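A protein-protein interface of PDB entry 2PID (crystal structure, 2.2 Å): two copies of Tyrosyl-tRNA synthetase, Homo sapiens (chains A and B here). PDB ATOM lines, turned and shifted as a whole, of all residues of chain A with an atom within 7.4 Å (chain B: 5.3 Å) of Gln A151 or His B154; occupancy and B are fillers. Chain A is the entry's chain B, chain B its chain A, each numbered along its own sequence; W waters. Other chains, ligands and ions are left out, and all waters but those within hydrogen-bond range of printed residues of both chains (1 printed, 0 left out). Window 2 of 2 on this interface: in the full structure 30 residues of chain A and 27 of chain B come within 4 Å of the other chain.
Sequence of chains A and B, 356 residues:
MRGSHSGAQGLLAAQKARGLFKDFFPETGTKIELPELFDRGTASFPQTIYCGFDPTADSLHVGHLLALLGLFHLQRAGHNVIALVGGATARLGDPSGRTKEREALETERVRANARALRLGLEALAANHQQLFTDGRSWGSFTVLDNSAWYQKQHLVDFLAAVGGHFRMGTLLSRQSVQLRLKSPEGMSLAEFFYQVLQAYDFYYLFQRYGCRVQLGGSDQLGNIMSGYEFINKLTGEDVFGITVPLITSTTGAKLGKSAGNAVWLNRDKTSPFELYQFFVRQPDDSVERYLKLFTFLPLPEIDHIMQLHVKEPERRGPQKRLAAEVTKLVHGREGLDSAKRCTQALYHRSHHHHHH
N of Leu A155 sits at hydrogen-bond distance from O of Gln B153 (2.9 Å). NE2 of His B154 sits close to O of Gln A151 (3.2 Å). The backbone NH of Leu B155 is in hydrogen-bond range of the backbone carbonyl oxygen of Gln A153, at 2.9 Å. The side-chain carboxylate of Asp B157 lies within salt-bridge range of the guanidinium group of Arg A91. N of Leu A155 sits close to N of Leu B155, 3.3 Å away.
The backbone NH of Ala A88 lies within hydrogen-bond range of the side-chain amide oxygen of Asn A146, at 2.9 Å.
Among the printed residues, merely in contact across the chains: Ala A88 with Val B156 (3.6 Å), Arg A91 with Val B156 (3.9 Å), Tyr A150 with Val B156 (3.9 Å), Gln A153 with His B154 (3.5 Å), His A154 with Gln B153 (3.4 Å), His A154 with His B154 (3.8 Å), His A154 with Leu B155 (3.8 Å), Leu A155 with His B154 (3.8 Å) and Leu A155 with Phe B158 (3.6 Å).
Printed residues of chain B within 4 Å of Ala A88: Val B156. Of the printed residues of chain B, Arg A91 touches Val B156 and Asp B157. Ser A147 touches none of the printed residues of chain B. Ala A148 touches none of the printed residues of chain B. Of the printed residues of chain B, Gln A153 touches His B154 (3.5 Å) and Leu B155 (2.9 Å). Of the printed residues of chain A, Gln B153 touches His A154 and Leu A155. Of the printed residues of chain A, Leu B155 touches Gln A153 (2.9 Å), His A154 (3.8 Å) and Leu A155 (3.3 Å). The nearest printed residue of chain B that does not touch Gln A151 is Val B156 (6.3 Å). The nearest residue of chain A that does not touch His B154 is Tyr A150 (4.5 Å). The nearest printed residue of chain B that does not touch Tyr A150 is Leu B155 (4.03 Å).
Hydrophobic or aromatic side chains of chain B within 4 Å of the printed part of chain A: His B154, Leu B155, Val B156 and Phe B158. Of the 14 printed residues of chain A, 7 touch a printed residue of chain B. Hydrophobic or aromatic side chains of chain A within 4 Å of the printed part of chain B: Tyr A150, His A154 and Leu A155. Among the printed residues, 14 pairs touch across the chains.
Gln A153 touches His B154, and with the chains exchanged His A154 touches Gln B153. Gln A153 touches Leu B155, and with the chains exchanged Leu A155 touches Gln B153. His B154 touches its own counterpart, His A154. His A154 touches Leu B155, and with the chains exchanged Leu A155 touches His B154. 5 positions are printed for both chains. Of the 14 pairs that touch across the chains among the printed residues, 8 have their exchanged pair printed and touching as well.
Water W1 lies within hydrogen-bond range of O of Tyr A150 (2.8 Å), N of Val B156 (2.8 Å) and N of Leu B155 (3.2 Å).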
ATOM      1  N   ALA A  88       1.977  31.937  13.115  1.00  0.00           N
ATOM      2  CA  ALA A  88       1.546  31.025  14.174  1.00  0.00           C
ATOM      3  C   ALA A  88       1.097  31.817  15.418  1.00  0.00           C
ATOM      4  O   ALA A  88       0.053  31.535  15.997  1.00  0.00           O
ATOM      5  CB  ALA A  88       2.713  30.038  14.557  1.00  0.00           C
ATOM      6  N   ARG A  91      -2.307  33.457  15.643  1.00  0.00           N
ATOM      7  CA  ARG A  91      -3.420  32.550  15.881  1.00  0.00           C
ATOM      8  C   ARG A  91      -3.868  32.629  17.338  1.00  0.00           C
ATOM      9  O   ARG A  91      -5.012  32.315  17.659  1.00  0.00           O
ATOM     10  CB  ARG A  91      -3.023  31.123  15.560  1.00  0.00           C
ATOM     11  CG  ARG A  91      -3.060  30.821  14.101  1.00  0.00           C
ATOM     12  CD  ARG A  91      -3.713  29.489  13.933  1.00  0.00           C
ATOM     13  NE  ARG A  91      -2.707  28.472  13.769  1.00  0.00           N
ATOM     14  CZ  ARG A  91      -2.926  27.175  13.905  1.00  0.00           C
ATOM     15  NH1 ARG A  91      -4.138  26.722  14.214  1.00  0.00           N
ATOM     16  NH2 ARG A  91      -1.915  26.341  13.725  1.00  0.00           N
ATOM     17  N   ARG A 111      -3.844  32.877   7.928  1.00  0.00           N
ATOM     18  CA  ARG A 111      -2.968  32.458   6.826  1.00  0.00           C
ATOM     19  C   ARG A 111      -2.932  33.478   5.671  1.00  0.00           C
ATOM     20  O   ARG A 111      -1.882  33.713   5.068  1.00  0.00           O
ATOM     21  CB  ARG A 111      -3.420  31.113   6.244  1.00  0.00           C
ATOM     22  CG  ARG A 111      -3.332  29.937   7.197  1.00  0.00           C
ATOM     23  CD  ARG A 111      -1.907  29.686   7.649  1.00  0.00           C
ATOM     24  NE  ARG A 111      -1.849  28.644   8.671  1.00  0.00           N
ATOM     25  CZ  ARG A 111      -0.967  28.623   9.667  1.00  0.00           C
ATOM     26  NH1 ARG A 111      -0.062  29.591   9.778  1.00  0.00           N
ATOM     27  NH2 ARG A 111      -0.997  27.642  10.560  1.00  0.00           N
ATOM     28  N   ASN A 146       6.992  32.413  11.346  1.00  0.00           N
ATOM     29  CA  ASN A 146       7.223  31.385  12.354  1.00  0.00           C
ATOM     30  C   ASN A 146       6.329  30.152  12.175  1.00  0.00           C
ATOM     31  O   ASN A 146       6.576  29.124  12.786  1.00  0.00           O
ATOM     32  CB  ASN A 146       7.161  31.944  13.801  1.00  0.00           C
ATOM     33  CG  ASN A 146       5.833  32.620  14.141  1.00  0.00           C
ATOM     34  OD1 ASN A 146       4.841  32.427  13.466  1.00  0.00           O
ATOM     35  ND2 ASN A 146       5.824  33.408  15.219  1.00  0.00           N
ATOM     36  N   SER A 147       5.299  30.243  11.335  1.00  0.00           N
ATOM     37  CA  SER A 147       4.483  29.061  11.095  1.00  0.00           C
ATOM     38  C   SER A 147       5.385  28.028  10.395  1.00  0.00           C
ATOM     39  O   SER A 147       5.115  26.833  10.427  1.00  0.00           O
ATOM     40  CB  SER A 147       3.285  29.381  10.200  1.00  0.00           C
ATOM     41  OG  SER A 147       3.738  29.676   8.899  1.00  0.00           O
ATOM     42  N   ALA A 148       6.466  28.491   9.775  1.00  0.00           N
ATOM     43  CA  ALA A 148       7.394  27.579   9.108  1.00  0.00           C
ATOM     44  C   ALA A 148       7.965  26.548  10.094  1.00  0.00           C
ATOM     45  O   ALA A 148       8.076  25.378   9.756  1.00  0.00           O
ATOM     46  CB  ALA A 148       8.534  28.362   8.442  1.00  0.00           C
ATOM     47  N   TRP A 149       8.340  26.958  11.308  1.00  0.00           N
ATOM     48  CA  TRP A 149       8.844  25.959  12.250  1.00  0.00           C
ATOM     49  C   TRP A 149       7.773  25.397  13.182  1.00  0.00           C
ATOM     50  O   TRP A 149       7.857  24.236  13.567  1.00  0.00           O
ATOM     51  CB  TRP A 149      10.030  26.476  13.076  1.00  0.00           C
ATOM     52  CG  TRP A 149       9.903  27.863  13.668  1.00  0.00           C
ATOM     53  CD1 TRP A 149       9.459  28.193  14.931  1.00  0.00           C
ATOM     54  CD2 TRP A 149      10.315  29.091  13.055  1.00  0.00           C
ATOM     55  NE1 TRP A 149       9.589  29.548  15.135  1.00  0.00           N
ATOM     56  CE2 TRP A 149      10.107  30.124  14.002  1.00  0.00           C
ATOM     57  CE3 TRP A 149      10.844  29.418  11.793  1.00  0.00           C
ATOM     58  CZ2 TRP A 149      10.414  31.469  13.728  1.00  0.00           C
ATOM     59  CZ3 TRP A 149      11.145  30.755  11.523  1.00  0.00           C
ATOM     60  CH2 TRP A 149      10.929  31.764  12.492  1.00  0.00           C
ATOM     61  N   TYR A 150       6.750  26.180  13.526  1.00  0.00           N
ATOM     62  CA  TYR A 150       5.730  25.640  14.427  1.00  0.00           C
ATOM     63  C   TYR A 150       4.870  24.550  13.802  1.00  0.00           C
ATOM     64  O   TYR A 150       4.383  23.682  14.511  1.00  0.00           O
ATOM     65  CB  TYR A 150       4.825  26.742  14.988  1.00  0.00           C
ATOM     66  CG  TYR A 150       5.513  27.561  16.067  1.00  0.00           C
ATOM     67  CD1 TYR A 150       6.047  26.922  17.188  1.00  0.00           C
ATOM     68  CD2 TYR A 150       5.686  28.950  15.967  1.00  0.00           C
ATOM     69  CE1 TYR A 150       6.737  27.601  18.159  1.00  0.00           C
ATOM     70  CE2 TYR A 150       6.391  29.636  16.927  1.00  0.00           C
ATOM     71  CZ  TYR A 150       6.917  28.970  18.017  1.00  0.00           C
ATOM     72  OH  TYR A 150       7.615  29.683  18.967  1.00  0.00           O
ATOM     73  N   GLN A 151       4.676  24.590  12.488  1.00  0.00           N
ATOM     74  CA  GLN A 151       3.880  23.562  11.833  1.00  0.00           C
ATOM     75  C   GLN A 151       4.514  22.182  11.962  1.00  0.00           C
ATOM     76  O   GLN A 151       3.864  21.182  11.698  1.00  0.00           O
ATOM     77  CB  GLN A 151       3.683  23.892  10.354  1.00  0.00           C
ATOM     78  CG  GLN A 151       2.528  24.849  10.090  1.00  0.00           C
ATOM     79  CD  GLN A 151       2.427  25.226   8.622  1.00  0.00           C
ATOM     80  OE1 GLN A 151       1.438  25.818   8.193  1.00  0.00           O
ATOM     81  NE2 GLN A 151       3.459  24.893   7.848  1.00  0.00           N
ATOM     82  N   LYS A 152       5.779  22.132  12.373  1.00  0.00           N
ATOM     83  CA  LYS A 152       6.481  20.863  12.549  1.00  0.00           C
ATOM     84  C   LYS A 152       6.717  20.586  14.037  1.00  0.00           C
ATOM     85  O   LYS A 152       7.514  19.720  14.395  1.00  0.00           O
ATOM     86  CB  LYS A 152       7.839  20.895  11.825  1.00  0.00           C
ATOM     87  CG  LYS A 152       7.745  21.290  10.354  1.00  0.00           C
ATOM     88  CD  LYS A 152       6.891  20.306   9.576  1.00  0.00           C
ATOM     89  CE  LYS A 152       6.406  20.909   8.258  1.00  0.00           C
ATOM     90  NZ  LYS A 152       7.531  21.369   7.397  1.00  0.00           N
ATOM     91  N   GLN A 153       6.026  21.317  14.905  1.00  0.00           N
ATOM     92  CA  GLN A 153       6.217  21.139  16.345  1.00  0.00           C
ATOM     93  C   GLN A 153       5.015  20.496  16.979  1.00  0.00           C
ATOM     94  O   GLN A 153       3.935  21.093  17.013  1.00  0.00           O
ATOM     95  CB  GLN A 153       6.449  22.487  17.034  1.00  0.00           C
ATOM     96  CG  GLN A 153       7.867  23.011  17.038  1.00  0.00           C
ATOM     97  CD  GLN A 153       8.821  22.086  17.765  1.00  0.00           C
ATOM     98  OE1 GLN A 153       8.479  21.506  18.789  1.00  0.00           O
ATOM     99  NE2 GLN A 153      10.027  21.953  17.238  1.00  0.00           N
ATOM    100  N   HIS A 154       5.173  19.287  17.491  1.00  0.00           N
ATOM    101  CA  HIS A 154       4.029  18.672  18.141  1.00  0.00           C
ATOM    102  C   HIS A 154       3.989  19.151  19.583  1.00  0.00           C
ATOM    103  O   HIS A 154       5.015  19.420  20.183  1.00  0.00           O
ATOM    104  CB  HIS A 154       4.092  17.139  18.080  1.00  0.00           C
ATOM    105  CG  HIS A 154       3.714  16.581  16.742  1.00  0.00           C
ATOM    106  ND1 HIS A 154       4.569  16.592  15.660  1.00  0.00           N
ATOM    107  CD2 HIS A 154       2.557  16.039  16.301  1.00  0.00           C
ATOM    108  CE1 HIS A 154       3.953  16.079  14.611  1.00  0.00           C
ATOM    109  NE2 HIS A 154       2.732  15.736  14.973  1.00  0.00           N
ATOM    110  N   LEU A 155       2.787  19.268  20.113  1.00  0.00           N
ATOM    111  CA  LEU A 155       2.554  19.720  21.477  1.00  0.00           C
ATOM    112  C   LEU A 155       3.471  19.123  22.550  1.00  0.00           C
ATOM    113  O   LEU A 155       4.222  19.836  23.210  1.00  0.00           O
ATOM    114  CB  LEU A 155       1.102  19.433  21.838  1.00  0.00           C
ATOM    115  CG  LEU A 155       0.661  19.761  23.261  1.00  0.00           C
ATOM    116  CD1 LEU A 155       0.683  21.290  23.469  1.00  0.00           C
ATOM    117  CD2 LEU A 155      -0.746  19.176  23.481  1.00  0.00           C
ATOM    118  N   VAL A 156       3.420  17.810  22.721  1.00  0.00           N
ATOM    119  CA  VAL A 156       4.225  17.162  23.741  1.00  0.00           C
ATOM    120  C   VAL A 156       5.716  17.175  23.476  1.00  0.00           C
ATOM    121  O   VAL A 156       6.514  17.330  24.411  1.00  0.00           O
ATOM    122  CB  VAL A 156       3.732  15.736  23.987  1.00  0.00           C
ATOM    123  CG1 VAL A 156       4.500  15.117  25.147  1.00  0.00           C
ATOM    124  CG2 VAL A 156       2.240  15.785  24.327  1.00  0.00           C
ATOM    125  N   LYS B 152      -0.589  13.454  17.188  1.00  0.00           N
ATOM    126  CA  LYS B 152      -1.231  14.111  16.056  1.00  0.00           C
ATOM    127  C   LYS B 152      -1.553  15.552  16.422  1.00  0.00           C
ATOM    128  O   LYS B 152      -2.093  16.304  15.610  1.00  0.00           O
ATOM    129  CB  LYS B 152      -2.526  13.384  15.675  1.00  0.00           C
ATOM    130  CG  LYS B 152      -2.358  11.872  15.470  1.00  0.00           C
ATOM    131  CD  LYS B 152      -3.496  11.257  14.635  1.00  0.00           C
ATOM    132  CE  LYS B 152      -4.875  11.472  15.247  1.00  0.00           C
ATOM    133  NZ  LYS B 152      -5.100  10.679  16.495  1.00  0.00           N
ATOM    134  N   GLN B 153      -1.227  15.931  17.654  1.00  0.00           N
ATOM    135  CA  GLN B 153      -1.494  17.280  18.132  1.00  0.00           C
ATOM    136  C   GLN B 153      -0.327  18.229  17.932  1.00  0.00           C
ATOM    137  O   GLN B 153       0.741  18.023  18.502  1.00  0.00           O
ATOM    138  CB  GLN B 153      -1.836  17.267  19.620  1.00  0.00           C
ATOM    139  CG  GLN B 153      -3.301  17.174  19.922  1.00  0.00           C
ATOM    140  CD  GLN B 153      -4.086  18.227  19.182  1.00  0.00           C
ATOM    141  OE1 GLN B 153      -3.685  19.391  19.120  1.00  0.00           O
ATOM    142  NE2 GLN B 153      -5.215  17.825  18.608  1.00  0.00           N
ATOM    143  N   HIS B 154      -0.518  19.262  17.117  1.00  0.00           N
ATOM    144  CA  HIS B 154       0.549  20.238  16.923  1.00  0.00           C
ATOM    145  C   HIS B 154       0.416  21.310  18.003  1.00  0.00           C
ATOM    146  O   HIS B 154      -0.683  21.607  18.476  1.00  0.00           O
ATOM    147  CB  HIS B 154       0.485  20.864  15.533  1.00  0.00           C
ATOM    148  CG  HIS B 154       0.973  19.957  14.443  1.00  0.00           C
ATOM    149  ND1 HIS B 154       0.186  18.976  13.878  1.00  0.00           N
ATOM    150  CD2 HIS B 154       2.175  19.874  13.825  1.00  0.00           C
ATOM    151  CE1 HIS B 154       0.880  18.329  12.958  1.00  0.00           C
ATOM    152  NE2 HIS B 154       2.090  18.853  12.906  1.00  0.00           N
ATOM    153  N   LEU B 155       1.552  21.860  18.405  1.00  0.00           N
ATOM    154  CA  LEU B 155       1.618  22.887  19.435  1.00  0.00           C
ATOM    155  C   LEU B 155       0.556  23.976  19.351  1.00  0.00           C
ATOM    156  O   LEU B 155      -0.318  24.090  20.223  1.00  0.00           O
ATOM    157  CB  LEU B 155       2.980  23.594  19.405  1.00  0.00           C
ATOM    158  CG  LEU B 155       3.660  23.941  20.733  1.00  0.00           C
ATOM    159  CD1 LEU B 155       4.644  25.085  20.512  1.00  0.00           C
ATOM    160  CD2 LEU B 155       2.645  24.303  21.802  1.00  0.00           C
ATOM    161  N   VAL B 156       0.658  24.781  18.299  1.00  0.00           N
ATOM    162  CA  VAL B 156      -0.216  25.921  18.115  1.00  0.00           C
ATOM    163  C   VAL B 156      -1.652  25.570  17.820  1.00  0.00           C
ATOM    164  O   VAL B 156      -2.555  26.292  18.230  1.00  0.00           O
ATOM    165  CB  VAL B 156       0.345  26.897  17.039  1.00  0.00           C
ATOM    166  CG1 VAL B 156      -0.478  28.170  17.014  1.00  0.00           C
ATOM    167  CG2 VAL B 156       1.782  27.250  17.376  1.00  0.00           C
ATOM    168  N   ASP B 157      -1.879  24.465  17.126  1.00  0.00           N
ATOM    169  CA  ASP B 157      -3.248  24.051  16.861  1.00  0.00           C
ATOM    170  C   ASP B 157      -3.949  23.778  18.190  1.00  0.00           C
ATOM    171  O   ASP B 157      -5.082  24.191  18.398  1.00  0.00           O
ATOM    172  CB  ASP B 157      -3.276  22.797  15.980  1.00  0.00           C
ATOM    173  CG  ASP B 157      -2.785  23.075  14.573  1.00  0.00           C
ATOM    174  OD1 ASP B 157      -3.130  24.147  14.039  1.00  0.00           O
ATOM    175  OD2 ASP B 157      -2.063  22.231  13.996  1.00  0.00           O
ATOM    176  N   PHE B 158      -3.256  23.092  19.089  1.00  0.00           N
ATOM    177  CA  PHE B 158      -3.806  22.766  20.395  1.00  0.00           C
ATOM    178  C   PHE B 158      -4.078  24.032  21.198  1.00  0.00           C
ATOM    179  O   PHE B 158      -5.161  24.199  21.758  1.00  0.00           O
ATOM    180  CB  PHE B 158      -2.825  21.879  21.173  1.00  0.00           C
ATOM    181  CG  PHE B 158      -3.326  21.457  22.524  1.00  0.00           C
ATOM    182  CD1 PHE B 158      -4.123  20.323  22.666  1.00  0.00           C
ATOM    183  CD2 PHE B 158      -2.988  22.186  23.663  1.00  0.00           C
ATOM    184  CE1 PHE B 158      -4.580  19.911  23.936  1.00  0.00           C
ATOM    185  CE2 PHE B 158      -3.431  21.789  24.928  1.00  0.00           C
ATOM    186  CZ  PHE B 158      -4.234  20.644  25.063  1.00  0.00           C
ATOM    187  N   LEU B 159      -3.092  24.924  21.260  1.00  0.00           N
ATOM    188  CA  LEU B 159      -3.250  26.155  22.028  1.00  0.00           C
ATOM    189  C   LEU B 159      -4.344  27.049  21.470  1.00  0.00           C
ATOM    190  O   LEU B 159      -4.994  27.775  22.219  1.00  0.00           O
ATOM    191  CB  LEU B 159      -1.938  26.936  22.065  1.00  0.00           C
ATOM    192  CG  LEU B 159      -0.818  26.296  22.881  1.00  0.00           C
ATOM    193  CD1 LEU B 159       0.508  26.932  22.496  1.00  0.00           C
ATOM    194  CD2 LEU B 159      -1.090  26.461  24.375  1.00  0.00           C
HETATM  195  O   HOH W   1       2.112  23.987  16.068  1.00  0.00           O
